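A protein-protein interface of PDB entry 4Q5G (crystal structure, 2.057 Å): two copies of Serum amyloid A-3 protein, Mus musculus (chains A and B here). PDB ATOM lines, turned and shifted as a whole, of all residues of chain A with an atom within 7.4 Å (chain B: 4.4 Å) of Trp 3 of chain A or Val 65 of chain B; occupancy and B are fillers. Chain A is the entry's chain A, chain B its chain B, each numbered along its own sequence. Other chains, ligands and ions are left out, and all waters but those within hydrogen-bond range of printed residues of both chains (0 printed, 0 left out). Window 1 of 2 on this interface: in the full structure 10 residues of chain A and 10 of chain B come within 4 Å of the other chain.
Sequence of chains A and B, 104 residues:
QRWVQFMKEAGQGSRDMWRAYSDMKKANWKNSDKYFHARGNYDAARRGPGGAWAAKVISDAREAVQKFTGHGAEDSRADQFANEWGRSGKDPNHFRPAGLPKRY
Among the printed residues, pairs that only touch across the chains: Trp 3 of chain A with Tyr 21 of chain B, Trp 3 of chain A with Arg 62 of chain B, Trp 53 of chain A with Ala 61 of chain B and Trp 3 of chain A with Val 65 of chain B.
Of chain B, only Tyr 21, Arg 62 and Val 65 come within 4 Å of Trp 3 of chain A. Of chain A, only Trp 3 comes within 4 Å of Val 65 of chain B. No residue of chain A comes within 4 Å of Ala 64 of chain B. Of the printed residues of chain A, Ala 61 of chain B touches Trp 53 (3.8 Å). Of the printed residues of chain B, Trp 53 of chain A touches Ala 61. Of the printed residues of chain A, Arg 62 of chain B touches Trp 3. Printed residues of chain A within 4 Å of Tyr 21 of chain B: Trp 3. Arg 2 of chain A touches none of the printed residues of chain B. The nearest residue of chain B that does not touch Trp 3 of chain A is Ala 61 of chain B (4.2 Å).
Printed residues of chain A that touch a printed residue of chain B: Trp 3 and Trp 53. Among the printed residues, no Asp or Glu carboxylate lies within 4 Å of a Lys or Arg side-chain nitrogen of the other chain.
No position is printed for both chains. Of the 4 pairs that touch across the chains among the printed residues, none has its exchanged pair printed and touching as well.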
ATOM      1  N   ARG A   2      12.453   4.851  20.804  1.00  0.00           N
ATOM      2  CA  ARG A   2      11.836   3.708  20.153  1.00  0.00           C
ATOM      3  C   ARG A   2      12.755   3.065  19.107  1.00  0.00           C
ATOM      4  O   ARG A   2      13.406   3.740  18.316  1.00  0.00           O
ATOM      5  CB  ARG A   2      10.508   4.101  19.496  1.00  0.00           C
ATOM      6  CG  ARG A   2       9.350   4.339  20.469  1.00  0.00           C
ATOM      7  CD  ARG A   2       8.676   3.047  20.908  1.00  0.00           C
ATOM      8  NE  ARG A   2       9.438   2.328  21.927  1.00  0.00           N
ATOM      9  CZ  ARG A   2      10.193   1.260  21.684  1.00  0.00           C
ATOM     10  NH1 ARG A   2      10.291   0.784  20.449  1.00  0.00           N
ATOM     11  NH2 ARG A   2      10.858   0.673  22.674  1.00  0.00           N
ATOM     12  N   TRP A   3      12.783   1.741  19.142  1.00  0.00           N
ATOM     13  CA  TRP A   3      13.423   0.918  18.137  1.00  0.00           C
ATOM     14  C   TRP A   3      12.675   1.066  16.821  1.00  0.00           C
ATOM     15  O   TRP A   3      13.266   1.031  15.743  1.00  0.00           O
ATOM     16  CB  TRP A   3      13.442  -0.543  18.602  1.00  0.00           C
ATOM     17  CG  TRP A   3      14.032  -1.521  17.627  1.00  0.00           C
ATOM     18  CD1 TRP A   3      13.392  -2.563  17.035  1.00  0.00           C
ATOM     19  CD2 TRP A   3      15.379  -1.546  17.136  1.00  0.00           C
ATOM     20  NE1 TRP A   3      14.250  -3.240  16.208  1.00  0.00           N
ATOM     21  CE2 TRP A   3      15.477  -2.632  16.245  1.00  0.00           C
ATOM     22  CE3 TRP A   3      16.508  -0.748  17.354  1.00  0.00           C
ATOM     23  CZ2 TRP A   3      16.653  -2.952  15.585  1.00  0.00           C
ATOM     24  CZ3 TRP A   3      17.675  -1.061  16.694  1.00  0.00           C
ATOM     25  CH2 TRP A   3      17.741  -2.155  15.820  1.00  0.00           C
ATOM     26  N   VAL A   4      11.364   1.233  16.930  1.00  0.00           N
ATOM     27  CA  VAL A   4      10.507   1.426  15.769  1.00  0.00           C
ATOM     28  C   VAL A   4      10.911   2.688  15.026  1.00  0.00           C
ATOM     29  O   VAL A   4      11.114   2.679  13.814  1.00  0.00           O
ATOM     30  CB  VAL A   4       9.033   1.513  16.188  1.00  0.00           C
ATOM     31  CG1 VAL A   4       8.132   1.642  14.973  1.00  0.00           C
ATOM     32  CG2 VAL A   4       8.668   0.299  16.997  1.00  0.00           C
ATOM     33  N   GLN A   5      11.025   3.771  15.780  1.00  0.00           N
ATOM     34  CA  GLN A   5      11.453   5.052  15.257  1.00  0.00           C
ATOM     35  C   GLN A   5      12.813   4.916  14.578  1.00  0.00           C
ATOM     36  O   GLN A   5      13.030   5.449  13.489  1.00  0.00           O
ATOM     37  CB  GLN A   5      11.515   6.080  16.387  1.00  0.00           C
ATOM     38  CG  GLN A   5      11.838   7.481  15.943  1.00  0.00           C
ATOM     39  CD  GLN A   5      10.757   8.069  15.065  1.00  0.00           C
ATOM     40  OE1 GLN A   5      11.047   8.788  14.109  1.00  0.00           O
ATOM     41  NE2 GLN A   5       9.499   7.768  15.384  1.00  0.00           N
ATOM     42  N   PHE A   6      13.727   4.198  15.228  1.00  0.00           N
ATOM     43  CA  PHE A   6      15.063   3.971  14.689  1.00  0.00           C
ATOM     44  C   PHE A   6      15.010   3.270  13.331  1.00  0.00           C
ATOM     45  O   PHE A   6      15.653   3.710  12.379  1.00  0.00           O
ATOM     46  CB  PHE A   6      15.898   3.149  15.677  1.00  0.00           C
ATOM     47  CG  PHE A   6      17.327   2.983  15.280  1.00  0.00           C
ATOM     48  CD1 PHE A   6      18.270   3.934  15.632  1.00  0.00           C
ATOM     49  CD2 PHE A   6      17.740   1.867  14.564  1.00  0.00           C
ATOM     50  CE1 PHE A   6      19.599   3.779  15.274  1.00  0.00           C
ATOM     51  CE2 PHE A   6      19.063   1.705  14.199  1.00  0.00           C
ATOM     52  CZ  PHE A   6      19.997   2.664  14.554  1.00  0.00           C
ATOM     53  N   MET A   7      14.239   2.188  13.239  1.00  0.00           N
ATOM     54  CA  MET A   7      14.169   1.418  11.997  1.00  0.00           C
ATOM     55  C   MET A   7      13.502   2.253  10.904  1.00  0.00           C
ATOM     56  O   MET A   7      13.902   2.199   9.735  1.00  0.00           O
ATOM     57  CB  MET A   7      13.411   0.102  12.198  1.00  0.00           C
ATOM     58  CG  MET A   7      14.191  -0.948  12.961  1.00  0.00           C
ATOM     59  SD  MET A   7      15.815  -1.531  11.999  1.00  0.00           S
ATOM     60  CE  MET A   7      14.989  -2.661  10.625  1.00  0.00           C
ATOM     61  N   LYS A   8      12.506   3.036  11.299  1.00  0.00           N
ATOM     62  CA  LYS A   8      11.816   3.935  10.381  1.00  0.00           C
ATOM     63  C   LYS A   8      12.783   4.959   9.787  1.00  0.00           C
ATOM     64  O   LYS A   8      12.829   5.155   8.576  1.00  0.00           O
ATOM     65  CB  LYS A   8      10.666   4.636  11.101  1.00  0.00           C
ATOM     66  CG  LYS A   8      10.217   5.941  10.459  1.00  0.00           C
ATOM     67  CD  LYS A   8       8.952   6.475  11.138  1.00  0.00           C
ATOM     68  CE  LYS A   8       8.758   7.967  10.897  1.00  0.00           C
ATOM     69  NZ  LYS A   8       9.797   8.794  11.582  1.00  0.00           N
ATOM     70  N   GLU A   9      13.574   5.595  10.641  1.00  0.00           N
ATOM     71  CA  GLU A   9      14.551   6.573  10.175  1.00  0.00           C
ATOM     72  C   GLU A   9      15.621   5.907   9.318  1.00  0.00           C
ATOM     73  O   GLU A   9      16.113   6.500   8.359  1.00  0.00           O
ATOM     74  CB  GLU A   9      15.192   7.301  11.359  1.00  0.00           C
ATOM     75  CG  GLU A   9      14.205   8.177  12.141  1.00  0.00           C
ATOM     76  CD  GLU A   9      14.716   8.560  13.526  1.00  0.00           C
ATOM     77  OE1 GLU A   9      15.813   8.095  13.926  1.00  0.00           O
ATOM     78  OE2 GLU A   9      14.009   9.314  14.227  1.00  0.00           O
ATOM     79  N   TRP A  53      22.800   6.135  11.180  1.00  0.00           N
ATOM     80  CA  TRP A  53      23.303   4.769  11.265  1.00  0.00           C
ATOM     81  C   TRP A  53      23.245   4.110   9.891  1.00  0.00           C
ATOM     82  O   TRP A  53      24.231   3.538   9.425  1.00  0.00           O
ATOM     83  CB  TRP A  53      22.511   3.943  12.285  1.00  0.00           C
ATOM     84  CG  TRP A  53      22.859   2.486  12.217  1.00  0.00           C
ATOM     85  CD1 TRP A  53      23.918   1.867  12.814  1.00  0.00           C
ATOM     86  CD2 TRP A  53      22.155   1.477  11.496  1.00  0.00           C
ATOM     87  NE1 TRP A  53      23.914   0.527  12.511  1.00  0.00           N
ATOM     88  CE2 TRP A  53      22.844   0.264  11.694  1.00  0.00           C
ATOM     89  CE3 TRP A  53      21.003   1.478  10.702  1.00  0.00           C
ATOM     90  CZ2 TRP A  53      22.412  -0.945  11.137  1.00  0.00           C
ATOM     91  CZ3 TRP A  53      20.580   0.284  10.141  1.00  0.00           C
ATOM     92  CH2 TRP A  53      21.282  -0.911  10.361  1.00  0.00           C
ATOM     93  N   TYR B  21      11.003  -8.818  13.792  1.00  0.00           N
ATOM     94  CA  TYR B  21      10.797  -8.018  14.994  1.00  0.00           C
ATOM     95  C   TYR B  21       9.327  -7.907  15.328  1.00  0.00           C
ATOM     96  O   TYR B  21       8.899  -8.192  16.450  1.00  0.00           O
ATOM     97  CB  TYR B  21      11.382  -6.621  14.824  1.00  0.00           C
ATOM     98  CG  TYR B  21      11.107  -5.730  16.014  1.00  0.00           C
ATOM     99  CD1 TYR B  21      11.776  -5.928  17.218  1.00  0.00           C
ATOM    100  CD2 TYR B  21      10.174  -4.702  15.941  1.00  0.00           C
ATOM    101  CE1 TYR B  21      11.525  -5.124  18.320  1.00  0.00           C
ATOM    102  CE2 TYR B  21       9.924  -3.879  17.038  1.00  0.00           C
ATOM    103  CZ  TYR B  21      10.603  -4.104  18.229  1.00  0.00           C
ATOM    104  OH  TYR B  21      10.363  -3.309  19.331  1.00  0.00           O
ATOM    105  N   ALA B  61      23.282  -3.838  15.325  1.00  0.00           N
ATOM    106  CA  ALA B  61      22.659  -2.623  15.867  1.00  0.00           C
ATOM    107  C   ALA B  61      21.671  -2.955  16.969  1.00  0.00           C
ATOM    108  O   ALA B  61      21.626  -2.288  18.008  1.00  0.00           O
ATOM    109  CB  ALA B  61      21.948  -1.822  14.757  1.00  0.00           C
ATOM    110  N   ARG B  62      20.850  -3.967  16.729  1.00  0.00           N
ATOM    111  CA  ARG B  62      19.895  -4.409  17.732  1.00  0.00           C
ATOM    112  C   ARG B  62      20.610  -4.845  19.022  1.00  0.00           C
ATOM    113  O   ARG B  62      20.179  -4.502  20.128  1.00  0.00           O
ATOM    114  CB  ARG B  62      19.041  -5.555  17.174  1.00  0.00           C
ATOM    115  CG  ARG B  62      18.124  -6.207  18.178  1.00  0.00           C
ATOM    116  CD  ARG B  62      17.026  -5.261  18.636  1.00  0.00           C
ATOM    117  NE  ARG B  62      16.076  -5.936  19.517  1.00  0.00           N
ATOM    118  CZ  ARG B  62      15.038  -5.342  20.099  1.00  0.00           C
ATOM    119  NH1 ARG B  62      14.808  -4.054  19.893  1.00  0.00           N
ATOM    120  NH2 ARG B  62      14.232  -6.041  20.885  1.00  0.00           N
ATOM    121  N   GLU B  63      21.706  -5.585  18.869  1.00  0.00           N
ATOM    122  CA  GLU B  63      22.476  -6.084  20.008  1.00  0.00           C
ATOM    123  C   GLU B  63      23.050  -4.909  20.779  1.00  0.00           C
ATOM    124  O   GLU B  63      22.964  -4.856  22.005  1.00  0.00           O
ATOM    125  CB  GLU B  63      23.611  -7.018  19.561  1.00  0.00           C
ATOM    126  CG  GLU B  63      24.368  -7.672  20.728  1.00  0.00           C
ATOM    127  CD  GLU B  63      25.885  -7.734  20.518  1.00  0.00           C
ATOM    128  OE1 GLU B  63      26.346  -8.437  19.589  1.00  0.00           O
ATOM    129  OE2 GLU B  63      26.621  -7.074  21.289  1.00  0.00           O
ATOM    130  N   ALA B  64      23.626  -3.965  20.039  1.00  0.00           N
ATOM    131  CA  ALA B  64      24.179  -2.752  20.622  1.00  0.00           C
ATOM    132  C   ALA B  64      23.140  -2.025  21.467  1.00  0.00           C
ATOM    133  O   ALA B  64      23.326  -1.871  22.675  1.00  0.00           O
ATOM    134  CB  ALA B  64      24.708  -1.845  19.535  1.00  0.00           C
ATOM    135  N   VAL B  65      22.044  -1.599  20.838  1.00  0.00           N
ATOM    136  CA  VAL B  65      20.973  -0.872  21.530  1.00  0.00           C
ATOM    137  C   VAL B  65      20.433  -1.616  22.764  1.00  0.00           C
ATOM    138  O   VAL B  65      20.051  -0.995  23.752  1.00  0.00           O
ATOM    139  CB  VAL B  65      19.790  -0.563  20.577  1.00  0.00           C
ATOM    140  CG1 VAL B  65      18.687   0.178  21.312  1.00  0.00           C
ATOM    141  CG2 VAL B  65      20.253   0.274  19.416  1.00  0.00           C
ATOM    142  N   GLN B  66      20.414  -2.942  22.721  1.00  0.00           N
ATOM    143  CA  GLN B  66      19.953  -3.707  23.882  1.00  0.00           C
ATOM    144  C   GLN B  66      20.991  -3.719  25.001  1.00  0.00           C
ATOM    145  O   GLN B  66      20.649  -3.906  26.159  1.00  0.00           O
ATOM    146  CB  GLN B  66      19.601  -5.135  23.483  1.00  0.00           C
ATOM    147  CG  GLN B  66      18.344  -5.228  22.656  1.00  0.00           C
ATOM    148  CD  GLN B  66      17.963  -6.658  22.349  1.00  0.00           C
ATOM    149  OE1 GLN B  66      18.629  -7.335  21.561  1.00  0.00           O
ATOM    150  NE2 GLN B  66      16.887  -7.129  22.967  1.00  0.00           N
ATOM    151  N   LYS B  67      22.260  -3.526  24.658  1.00  0.00           N
ATOM    152  CA  LYS B  67      23.282  -3.387  25.689  1.00  0.00           C
ATOM    153  C   LYS B  67      23.297  -1.940  26.175  1.00  0.00           C
ATOM    154  O   LYS B  67      23.894  -1.624  27.206  1.00  0.00           O
ATOM    155  CB  LYS B  67      24.658  -3.812  25.174  1.00  0.00           C
ATOM    156  CG  LYS B  67      24.707  -5.237  24.666  1.00  0.00           C
ATOM    157  CD  LYS B  67      24.047  -6.205  25.636  1.00  0.00           C
ATOM    158  CE  LYS B  67      24.896  -6.426  26.877  1.00  0.00           C
ATOM    159  NZ  LYS B  67      24.347  -7.500  27.765  1.00  0.00           N
ATOM    160  N   PHE B  68      22.639  -1.068  25.420  1.00  0.00           N
ATOM    161  CA  PHE B  68      22.307   0.267  25.896  1.00  0.00           C
ATOM    162  C   PHE B  68      21.025   0.169  26.718  1.00  0.00           C
ATOM    163  O   PHE B  68      20.137   1.004  26.585  1.00  0.00           O
ATOM    164  CB  PHE B  68      22.095   1.246  24.725  1.00  0.00           C
ATOM    165  CG  PHE B  68      23.357   1.838  24.154  1.00  0.00           C
ATOM    166  CD1 PHE B  68      24.109   1.141  23.219  1.00  0.00           C
ATOM    167  CD2 PHE B  68      23.768   3.111  24.525  1.00  0.00           C
ATOM    168  CE1 PHE B  68      25.263   1.690  22.682  1.00  0.00           C
ATOM    169  CE2 PHE B  68      24.920   3.666  23.993  1.00  0.00           C
ATOM    170  CZ  PHE B  68      25.668   2.955  23.071  1.00  0.00           C
ATOM    171  N   THR B  69      20.924  -0.869  27.540  1.00  0.00           N
ATOM    172  CA  THR B  69      19.684  -1.160  28.237  1.00  0.00           C
ATOM    173  C   THR B  69      19.397  -0.050  29.246  1.00  0.00           C
ATOM    174  O   THR B  69      20.138   0.161  30.210  1.00  0.00           O
ATOM    175  CB  THR B  69      19.717  -2.549  28.924  1.00  0.00           C
ATOM    176  OG1 THR B  69      18.499  -2.766  29.648  1.00  0.00           O
ATOM    177  CG2 THR B  69      20.927  -2.700  29.852  1.00  0.00           C
